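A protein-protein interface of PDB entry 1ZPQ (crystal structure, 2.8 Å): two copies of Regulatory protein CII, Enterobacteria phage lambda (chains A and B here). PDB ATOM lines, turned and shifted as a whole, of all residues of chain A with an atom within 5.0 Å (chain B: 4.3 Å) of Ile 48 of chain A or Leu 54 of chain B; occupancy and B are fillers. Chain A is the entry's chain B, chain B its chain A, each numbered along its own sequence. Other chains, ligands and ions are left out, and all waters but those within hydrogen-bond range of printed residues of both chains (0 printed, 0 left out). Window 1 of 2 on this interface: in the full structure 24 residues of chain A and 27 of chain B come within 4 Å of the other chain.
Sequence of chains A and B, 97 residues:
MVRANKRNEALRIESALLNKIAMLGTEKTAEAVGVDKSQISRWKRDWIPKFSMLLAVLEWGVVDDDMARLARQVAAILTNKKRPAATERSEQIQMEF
Phe 51 of chain B touches its own counterpart, Phe 51 of chain A.
3 positions are printed for both chains.
Of the 8 pairs that touch across the chains among the printed residues, 1 has its exchanged pair printed and touching as well.
Ile 48 of chain A touches just one residue of chain B: Leu 54.
Leu 54 of chain B touches just these residues of chain A: Val 33 and Ile 48.
Of the printed residues of chain A, Val 57 of chain B touches Val 33 (3.3 Å).
Of the printed residues of chain B, Val 33 of chain A touches Met 53 (3.9 Å), Leu 54 (3.5 Å) and Val 57 (3.3 Å).
Printed residues of chain B within 4 Å of Phe 51 of chain A: Phe 51.
Printed residues of chain B within 4 Å of Ile 21 of chain A: Leu 58 (3.9 Å).
Of the printed residues of chain A, Phe 51 of chain B touches Leu 17 and Phe 51.
The nearest residue of chain A that does not touch Leu 54 of chain B is Trp 43 of chain A (4.1 Å).
The nearest printed residue of chain B that does not touch Leu 17 of chain A is Leu 55 of chain B (4.1 Å).
Phe 51 of chain B touches Leu 17 of chain A (CE1 to CD1, 3.7 Å).
Leu 17 of chain A touches Leu 58 of chain B (CD2 to CD1, 3.9 Å).
Ile 21 of chain A touches Leu 58 of chain B.
Met 53 of chain B touches Val 33 of chain A (O to CG2, 3.9 Å).
Val 33 of chain A touches Leu 54 of chain B.
Val 57 of chain B touches Val 33 of chain A (CG2 to CG2, 3.3 Å).
Ile 48 of chain A touches Leu 54 of chain B (CD1 to CD2, 3.7 Å).
Phe 51 of chain B touches Phe 51 of chain A.
Hydrophobic or aromatic side chains of chain B that line the printed part of chain A: Phe 51, Leu 54, Val 57 and Leu 58.
Among the printed residues, 8 pairs touch across the chains.
Among the printed residues, no Asp or Glu carboxylate lies within 4 Å of a Lys or Arg side-chain nitrogen of the other chain.
The side-chain hydroxyl of Ser 52 of chain A is in hydrogen-bond range of the backbone carbonyl oxygen of Ile 48 of chain A.
The backbone carbonyl oxygen (O) of Trp 43 of chain A is in hydrogen-bond range of the backbone NH (N) of Ile 48 of chain A (2.9 Å).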
ATOM      1  N   GLU A  14      14.598 -32.172   3.079  1.00  0.00           N
ATOM      2  CA  GLU A  14      15.520 -31.133   3.546  1.00  0.00           C
ATOM      3  C   GLU A  14      16.424 -31.590   4.613  1.00  0.00           C
ATOM      4  O   GLU A  14      17.628 -31.260   4.605  1.00  0.00           O
ATOM      5  CB  GLU A  14      14.766 -29.953   4.136  1.00  0.00           C
ATOM      6  CG  GLU A  14      15.706 -28.943   4.729  1.00  0.00           C
ATOM      7  CD  GLU A  14      15.065 -27.642   5.034  1.00  0.00           C
ATOM      8  OE1 GLU A  14      14.618 -27.023   4.035  1.00  0.00           O
ATOM      9  OE2 GLU A  14      15.095 -27.215   6.248  1.00  0.00           O
ATOM     10  N   LEU A  17      18.996 -34.059   2.860  1.00  0.00           N
ATOM     11  CA  LEU A  17      20.039 -33.499   2.109  1.00  0.00           C
ATOM     12  C   LEU A  17      21.072 -32.805   3.017  1.00  0.00           C
ATOM     13  O   LEU A  17      22.260 -32.835   2.741  1.00  0.00           O
ATOM     14  CB  LEU A  17      19.453 -32.553   1.089  1.00  0.00           C
ATOM     15  CG  LEU A  17      18.445 -33.222   0.199  1.00  0.00           C
ATOM     16  CD1 LEU A  17      17.742 -32.234  -0.709  1.00  0.00           C
ATOM     17  CD2 LEU A  17      19.107 -34.335  -0.561  1.00  0.00           C
ATOM     18  N   LEU A  18      20.607 -32.190   4.104  1.00  0.00           N
ATOM     19  CA  LEU A  18      21.491 -31.413   4.986  1.00  0.00           C
ATOM     20  C   LEU A  18      22.378 -32.299   5.765  1.00  0.00           C
ATOM     21  O   LEU A  18      23.467 -31.898   6.130  1.00  0.00           O
ATOM     22  CB  LEU A  18      20.656 -30.585   5.996  1.00  0.00           C
ATOM     23  CG  LEU A  18      19.814 -29.453   5.382  1.00  0.00           C
ATOM     24  CD1 LEU A  18      18.806 -28.733   6.423  1.00  0.00           C
ATOM     25  CD2 LEU A  18      20.745 -28.471   4.673  1.00  0.00           C
ATOM     26  N   ILE A  21      25.088 -33.234   3.323  1.00  0.00           N
ATOM     27  CA  ILE A  21      25.957 -32.172   3.104  1.00  0.00           C
ATOM     28  C   ILE A  21      26.928 -32.115   4.335  1.00  0.00           C
ATOM     29  O   ILE A  21      28.159 -32.069   4.226  1.00  0.00           O
ATOM     30  CB  ILE A  21      25.147 -30.934   3.074  1.00  0.00           C
ATOM     31  CG1 ILE A  21      24.335 -30.861   1.819  1.00  0.00           C
ATOM     32  CG2 ILE A  21      26.010 -29.762   3.060  1.00  0.00           C
ATOM     33  CD1 ILE A  21      23.347 -29.734   1.751  1.00  0.00           C
ATOM     34  N   THR A  29      31.494 -29.972   0.119  1.00  0.00           N
ATOM     35  CA  THR A  29      30.307 -30.061  -0.655  1.00  0.00           C
ATOM     36  C   THR A  29      30.024 -28.721  -1.288  1.00  0.00           C
ATOM     37  O   THR A  29      29.608 -28.699  -2.445  1.00  0.00           O
ATOM     38  CB  THR A  29      29.104 -30.457   0.141  1.00  0.00           C
ATOM     39  OG1 THR A  29      29.404 -31.612   0.929  1.00  0.00           O
ATOM     40  CG2 THR A  29      27.927 -30.737  -0.778  1.00  0.00           C
ATOM     41  N   VAL A  33      29.952 -29.041  -5.260  1.00  0.00           N
ATOM     42  CA  VAL A  33      28.738 -28.545  -5.899  1.00  0.00           C
ATOM     43  C   VAL A  33      29.043 -27.100  -6.354  1.00  0.00           C
ATOM     44  O   VAL A  33      30.173 -26.658  -6.342  1.00  0.00           O
ATOM     45  CB  VAL A  33      27.628 -28.732  -4.846  1.00  0.00           C
ATOM     46  CG1 VAL A  33      26.463 -27.974  -5.079  1.00  0.00           C
ATOM     47  CG2 VAL A  33      27.286 -30.215  -4.777  1.00  0.00           C
ATOM     48  N   TRP A  43      22.196 -21.020   0.457  1.00  0.00           N
ATOM     49  CA  TRP A  43      22.202 -22.388  -0.010  1.00  0.00           C
ATOM     50  C   TRP A  43      21.286 -23.161   0.906  1.00  0.00           C
ATOM     51  O   TRP A  43      20.172 -23.525   0.572  1.00  0.00           O
ATOM     52  CB  TRP A  43      23.656 -22.891  -0.024  1.00  0.00           C
ATOM     53  CG  TRP A  43      23.933 -24.280  -0.549  1.00  0.00           C
ATOM     54  CD1 TRP A  43      23.422 -24.854  -1.673  1.00  0.00           C
ATOM     55  CD2 TRP A  43      24.835 -25.259   0.010  1.00  0.00           C
ATOM     56  NE1 TRP A  43      23.911 -26.129  -1.811  1.00  0.00           N
ATOM     57  CE2 TRP A  43      24.779 -26.387  -0.791  1.00  0.00           C
ATOM     58  CE3 TRP A  43      25.642 -25.308   1.147  1.00  0.00           C
ATOM     59  CZ2 TRP A  43      25.461 -27.527  -0.496  1.00  0.00           C
ATOM     60  CZ3 TRP A  43      26.336 -26.443   1.399  1.00  0.00           C
ATOM     61  CH2 TRP A  43      26.236 -27.539   0.578  1.00  0.00           C
ATOM     62  N   LYS A  44      21.696 -23.276   2.126  1.00  0.00           N
ATOM     63  CA  LYS A  44      20.930 -24.046   3.050  1.00  0.00           C
ATOM     64  C   LYS A  44      19.538 -23.494   3.363  1.00  0.00           C
ATOM     65  O   LYS A  44      18.701 -24.227   3.839  1.00  0.00           O
ATOM     66  CB  LYS A  44      21.765 -24.199   4.318  1.00  0.00           C
ATOM     67  CG  LYS A  44      23.183 -24.760   4.093  1.00  0.00           C
ATOM     68  CD  LYS A  44      23.681 -25.412   5.380  1.00  0.00           C
ATOM     69  CE  LYS A  44      24.975 -26.124   5.147  1.00  0.00           C
ATOM     70  NZ  LYS A  44      25.731 -26.510   6.374  1.00  0.00           N
ATOM     71  N   ASP A  46      17.319 -21.148   1.361  1.00  0.00           N
ATOM     72  CA  ASP A  46      16.335 -20.997   0.271  1.00  0.00           C
ATOM     73  C   ASP A  46      16.463 -22.287  -0.513  1.00  0.00           C
ATOM     74  O   ASP A  46      15.439 -22.909  -0.814  1.00  0.00           O
ATOM     75  CB  ASP A  46      16.687 -20.000  -0.897  1.00  0.00           C
ATOM     76  CG  ASP A  46      16.067 -18.615  -0.929  1.00  0.00           C
ATOM     77  OD1 ASP A  46      16.862 -17.653  -0.731  1.00  0.00           O
ATOM     78  OD2 ASP A  46      14.852 -18.460  -1.203  1.00  0.00           O
ATOM     79  N   TRP A  47      17.708 -22.659  -0.904  1.00  0.00           N
ATOM     80  CA  TRP A  47      17.844 -23.644  -1.992  1.00  0.00           C
ATOM     81  C   TRP A  47      17.596 -25.055  -1.499  1.00  0.00           C
ATOM     82  O   TRP A  47      16.676 -25.728  -1.943  1.00  0.00           O
ATOM     83  CB  TRP A  47      19.162 -23.532  -2.720  1.00  0.00           C
ATOM     84  CG  TRP A  47      19.457 -22.110  -3.145  1.00  0.00           C
ATOM     85  CD1 TRP A  47      18.548 -21.129  -3.331  1.00  0.00           C
ATOM     86  CD2 TRP A  47      20.751 -21.511  -3.422  1.00  0.00           C
ATOM     87  NE1 TRP A  47      19.180 -19.957  -3.665  1.00  0.00           N
ATOM     88  CE2 TRP A  47      20.530 -20.168  -3.730  1.00  0.00           C
ATOM     89  CE3 TRP A  47      22.070 -21.984  -3.433  1.00  0.00           C
ATOM     90  CZ2 TRP A  47      21.563 -19.287  -4.049  1.00  0.00           C
ATOM     91  CZ3 TRP A  47      23.105 -21.084  -3.742  1.00  0.00           C
ATOM     92  CH2 TRP A  47      22.840 -19.770  -4.046  1.00  0.00           C
ATOM     93  N   ILE A  48      18.323 -25.504  -0.525  1.00  0.00           N
ATOM     94  CA  ILE A  48      17.926 -26.787   0.020  1.00  0.00           C
ATOM     95  C   ILE A  48      16.362 -26.980   0.251  1.00  0.00           C
ATOM     96  O   ILE A  48      15.757 -27.968  -0.128  1.00  0.00           O
ATOM     97  CB  ILE A  48      18.678 -27.069   1.261  1.00  0.00           C
ATOM     98  CG1 ILE A  48      20.193 -27.028   1.027  1.00  0.00           C
ATOM     99  CG2 ILE A  48      18.261 -28.390   1.730  1.00  0.00           C
ATOM    100  CD1 ILE A  48      20.683 -28.002   0.194  1.00  0.00           C
ATOM    101  N   PRO A  49      15.722 -26.038   0.902  1.00  0.00           N
ATOM    102  CA  PRO A  49      14.327 -26.191   1.229  1.00  0.00           C
ATOM    103  C   PRO A  49      13.595 -26.203  -0.037  1.00  0.00           C
ATOM    104  O   PRO A  49      12.807 -27.070  -0.160  1.00  0.00           O
ATOM    105  CB  PRO A  49      14.017 -24.921   1.977  1.00  0.00           C
ATOM    106  CG  PRO A  49      15.294 -24.423   2.454  1.00  0.00           C
ATOM    107  CD  PRO A  49      16.191 -24.752   1.404  1.00  0.00           C
ATOM    108  N   LYS A  50      13.831 -25.286  -0.947  1.00  0.00           N
ATOM    109  CA  LYS A  50      13.109 -25.314  -2.177  1.00  0.00           C
ATOM    110  C   LYS A  50      13.257 -26.674  -3.033  1.00  0.00           C
ATOM    111  O   LYS A  50      12.270 -27.237  -3.541  1.00  0.00           O
ATOM    112  CB  LYS A  50      13.367 -23.996  -2.963  1.00  0.00           C
ATOM    113  CG  LYS A  50      12.385 -22.736  -2.516  1.00  0.00           C
ATOM    114  CD  LYS A  50      12.145 -21.622  -3.656  1.00  0.00           C
ATOM    115  CE  LYS A  50      10.796 -20.809  -3.519  1.00  0.00           C
ATOM    116  NZ  LYS A  50      10.194 -20.384  -4.853  1.00  0.00           N
ATOM    117  N   PHE A  51      14.449 -27.231  -3.128  1.00  0.00           N
ATOM    118  CA  PHE A  51      14.645 -28.429  -3.881  1.00  0.00           C
ATOM    119  C   PHE A  51      14.062 -29.540  -3.210  1.00  0.00           C
ATOM    120  O   PHE A  51      13.772 -30.519  -3.789  1.00  0.00           O
ATOM    121  CB  PHE A  51      16.135 -28.670  -4.132  1.00  0.00           C
ATOM    122  CG  PHE A  51      16.708 -27.693  -5.197  1.00  0.00           C
ATOM    123  CD1 PHE A  51      18.112 -27.477  -5.346  1.00  0.00           C
ATOM    124  CD2 PHE A  51      15.785 -26.911  -6.042  1.00  0.00           C
ATOM    125  CE1 PHE A  51      18.575 -26.561  -6.280  1.00  0.00           C
ATOM    126  CE2 PHE A  51      16.252 -26.019  -6.958  1.00  0.00           C
ATOM    127  CZ  PHE A  51      17.654 -25.838  -7.074  1.00  0.00           C
ATOM    128  N   SER A  52      13.950 -29.435  -1.927  1.00  0.00           N
ATOM    129  CA  SER A  52      13.349 -30.490  -1.142  1.00  0.00           C
ATOM    130  C   SER A  52      11.904 -30.627  -1.420  1.00  0.00           C
ATOM    131  O   SER A  52      11.390 -31.706  -1.315  1.00  0.00           O
ATOM    132  CB  SER A  52      13.514 -30.226   0.304  1.00  0.00           C
ATOM    133  OG  SER A  52      14.829 -30.529   0.587  1.00  0.00           O
ATOM    134  N   LYS B  50      22.123 -27.832 -10.783  1.00  0.00           N
ATOM    135  CA  LYS B  50      22.796 -27.656  -9.494  1.00  0.00           C
ATOM    136  C   LYS B  50      22.288 -28.662  -8.496  1.00  0.00           C
ATOM    137  O   LYS B  50      23.081 -29.329  -7.845  1.00  0.00           O
ATOM    138  CB  LYS B  50      22.569 -26.242  -8.966  1.00  0.00           C
ATOM    139  CG  LYS B  50      23.896 -25.562  -8.473  1.00  0.00           C
ATOM    140  CD  LYS B  50      23.817 -24.025  -8.486  1.00  0.00           C
ATOM    141  CE  LYS B  50      23.639 -23.502  -9.888  1.00  0.00           C
ATOM    142  NZ  LYS B  50      23.907 -22.033  -9.884  1.00  0.00           N
ATOM    143  N   PHE B  51      20.975 -28.772  -8.377  1.00  0.00           N
ATOM    144  CA  PHE B  51      20.406 -29.816  -7.591  1.00  0.00           C
ATOM    145  C   PHE B  51      20.786 -31.247  -7.956  1.00  0.00           C
ATOM    146  O   PHE B  51      20.827 -32.124  -7.140  1.00  0.00           O
ATOM    147  CB  PHE B  51      18.898 -29.729  -7.669  1.00  0.00           C
ATOM    148  CG  PHE B  51      18.115 -30.507  -6.532  1.00  0.00           C
ATOM    149  CD1 PHE B  51      18.693 -30.826  -5.296  1.00  0.00           C
ATOM    150  CD2 PHE B  51      16.767 -30.842  -6.731  1.00  0.00           C
ATOM    151  CE1 PHE B  51      17.958 -31.423  -4.328  1.00  0.00           C
ATOM    152  CE2 PHE B  51      16.068 -31.464  -5.758  1.00  0.00           C
ATOM    153  CZ  PHE B  51      16.642 -31.739  -4.571  1.00  0.00           C
ATOM    154  N   SER B  52      20.987 -31.466  -9.214  1.00  0.00           N
ATOM    155  CA  SER B  52      21.426 -32.746  -9.775  1.00  0.00           C
ATOM    156  C   SER B  52      22.814 -32.963  -9.395  1.00  0.00           C
ATOM    157  O   SER B  52      23.214 -34.091  -9.183  1.00  0.00           O
ATOM    158  CB  SER B  52      21.341 -32.701 -11.278  1.00  0.00           C
ATOM    159  OG  SER B  52      19.987 -32.391 -11.597  1.00  0.00           O
ATOM    160  N   MET B  53      23.568 -31.882  -9.368  1.00  0.00           N
ATOM    161  CA  MET B  53      24.981 -31.939  -9.058  1.00  0.00           C
ATOM    162  C   MET B  53      25.110 -32.221  -7.572  1.00  0.00           C
ATOM    163  O   MET B  53      25.876 -32.958  -7.195  1.00  0.00           O
ATOM    164  CB  MET B  53      25.642 -30.615  -9.466  1.00  0.00           C
ATOM    165  CG  MET B  53      27.207 -30.581  -9.387  1.00  0.00           C
ATOM    166  SD  MET B  53      27.903 -31.656 -10.640  1.00  0.00           S
ATOM    167  CE  MET B  53      28.333 -32.963  -9.639  1.00  0.00           C
ATOM    168  N   LEU B  54      24.287 -31.570  -6.752  1.00  0.00           N
ATOM    169  CA  LEU B  54      24.240 -31.785  -5.375  1.00  0.00           C
ATOM    170  C   LEU B  54      23.878 -33.243  -5.250  1.00  0.00           C
ATOM    171  O   LEU B  54      24.469 -33.971  -4.414  1.00  0.00           O
ATOM    172  CB  LEU B  54      23.127 -30.954  -4.760  1.00  0.00           C
ATOM    173  CG  LEU B  54      22.945 -31.060  -3.228  1.00  0.00           C
ATOM    174  CD1 LEU B  54      24.226 -30.735  -2.651  1.00  0.00           C
ATOM    175  CD2 LEU B  54      21.793 -30.197  -2.614  1.00  0.00           C
ATOM    176  N   LEU B  55      22.815 -33.658  -5.909  1.00  0.00           N
ATOM    177  CA  LEU B  55      22.499 -35.052  -5.882  1.00  0.00           C
ATOM    178  C   LEU B  55      23.704 -35.988  -6.377  1.00  0.00           C
ATOM    179  O   LEU B  55      23.889 -37.146  -5.988  1.00  0.00           O
ATOM    180  CB  LEU B  55      21.229 -35.341  -6.680  1.00  0.00           C
ATOM    181  CG  LEU B  55      19.994 -35.576  -5.890  1.00  0.00           C
ATOM    182  CD1 LEU B  55      19.918 -34.727  -4.583  1.00  0.00           C
ATOM    183  CD2 LEU B  55      18.809 -35.271  -6.747  1.00  0.00           C
ATOM    184  N   ALA B  56      24.505 -35.515  -7.253  1.00  0.00           N
ATOM    185  CA  ALA B  56      25.492 -36.415  -7.764  1.00  0.00           C
ATOM    186  C   ALA B  56      26.661 -36.425  -6.843  1.00  0.00           C
ATOM    187  O   ALA B  56      27.340 -37.391  -6.726  1.00  0.00           O
ATOM    188  CB  ALA B  56      25.861 -35.985  -9.156  1.00  0.00           C
ATOM    189  N   VAL B  57      26.836 -35.353  -6.089  1.00  0.00           N
ATOM    190  CA  VAL B  57      27.924 -35.236  -5.132  1.00  0.00           C
ATOM    191  C   VAL B  57      27.562 -35.961  -3.952  1.00  0.00           C
ATOM    192  O   VAL B  57      28.396 -36.667  -3.461  1.00  0.00           O
ATOM    193  CB  VAL B  57      28.223 -33.827  -4.663  1.00  0.00           C
ATOM    194  CG1 VAL B  57      29.214 -33.884  -3.489  1.00  0.00           C
ATOM    195  CG2 VAL B  57      28.738 -33.022  -5.792  1.00  0.00           C
ATOM    196  N   LEU B  58      26.338 -35.721  -3.549  1.00  0.00           N
ATOM    197  CA  LEU B  58      25.820 -36.411  -2.443  1.00  0.00           C
ATOM    198  C   LEU B  58      25.717 -37.834  -2.901  1.00  0.00           C
ATOM    199  O   LEU B  58      25.431 -38.713  -2.102  1.00  0.00           O
ATOM    200  CB  LEU B  58      24.461 -35.876  -1.968  1.00  0.00           C
ATOM    201  CG  LEU B  58      24.409 -34.429  -1.506  1.00  0.00           C
ATOM    202  CD1 LEU B  58      23.011 -34.073  -1.005  1.00  0.00           C
ATOM    203  CD2 LEU B  58      25.442 -34.163  -0.429  1.00  0.00           C
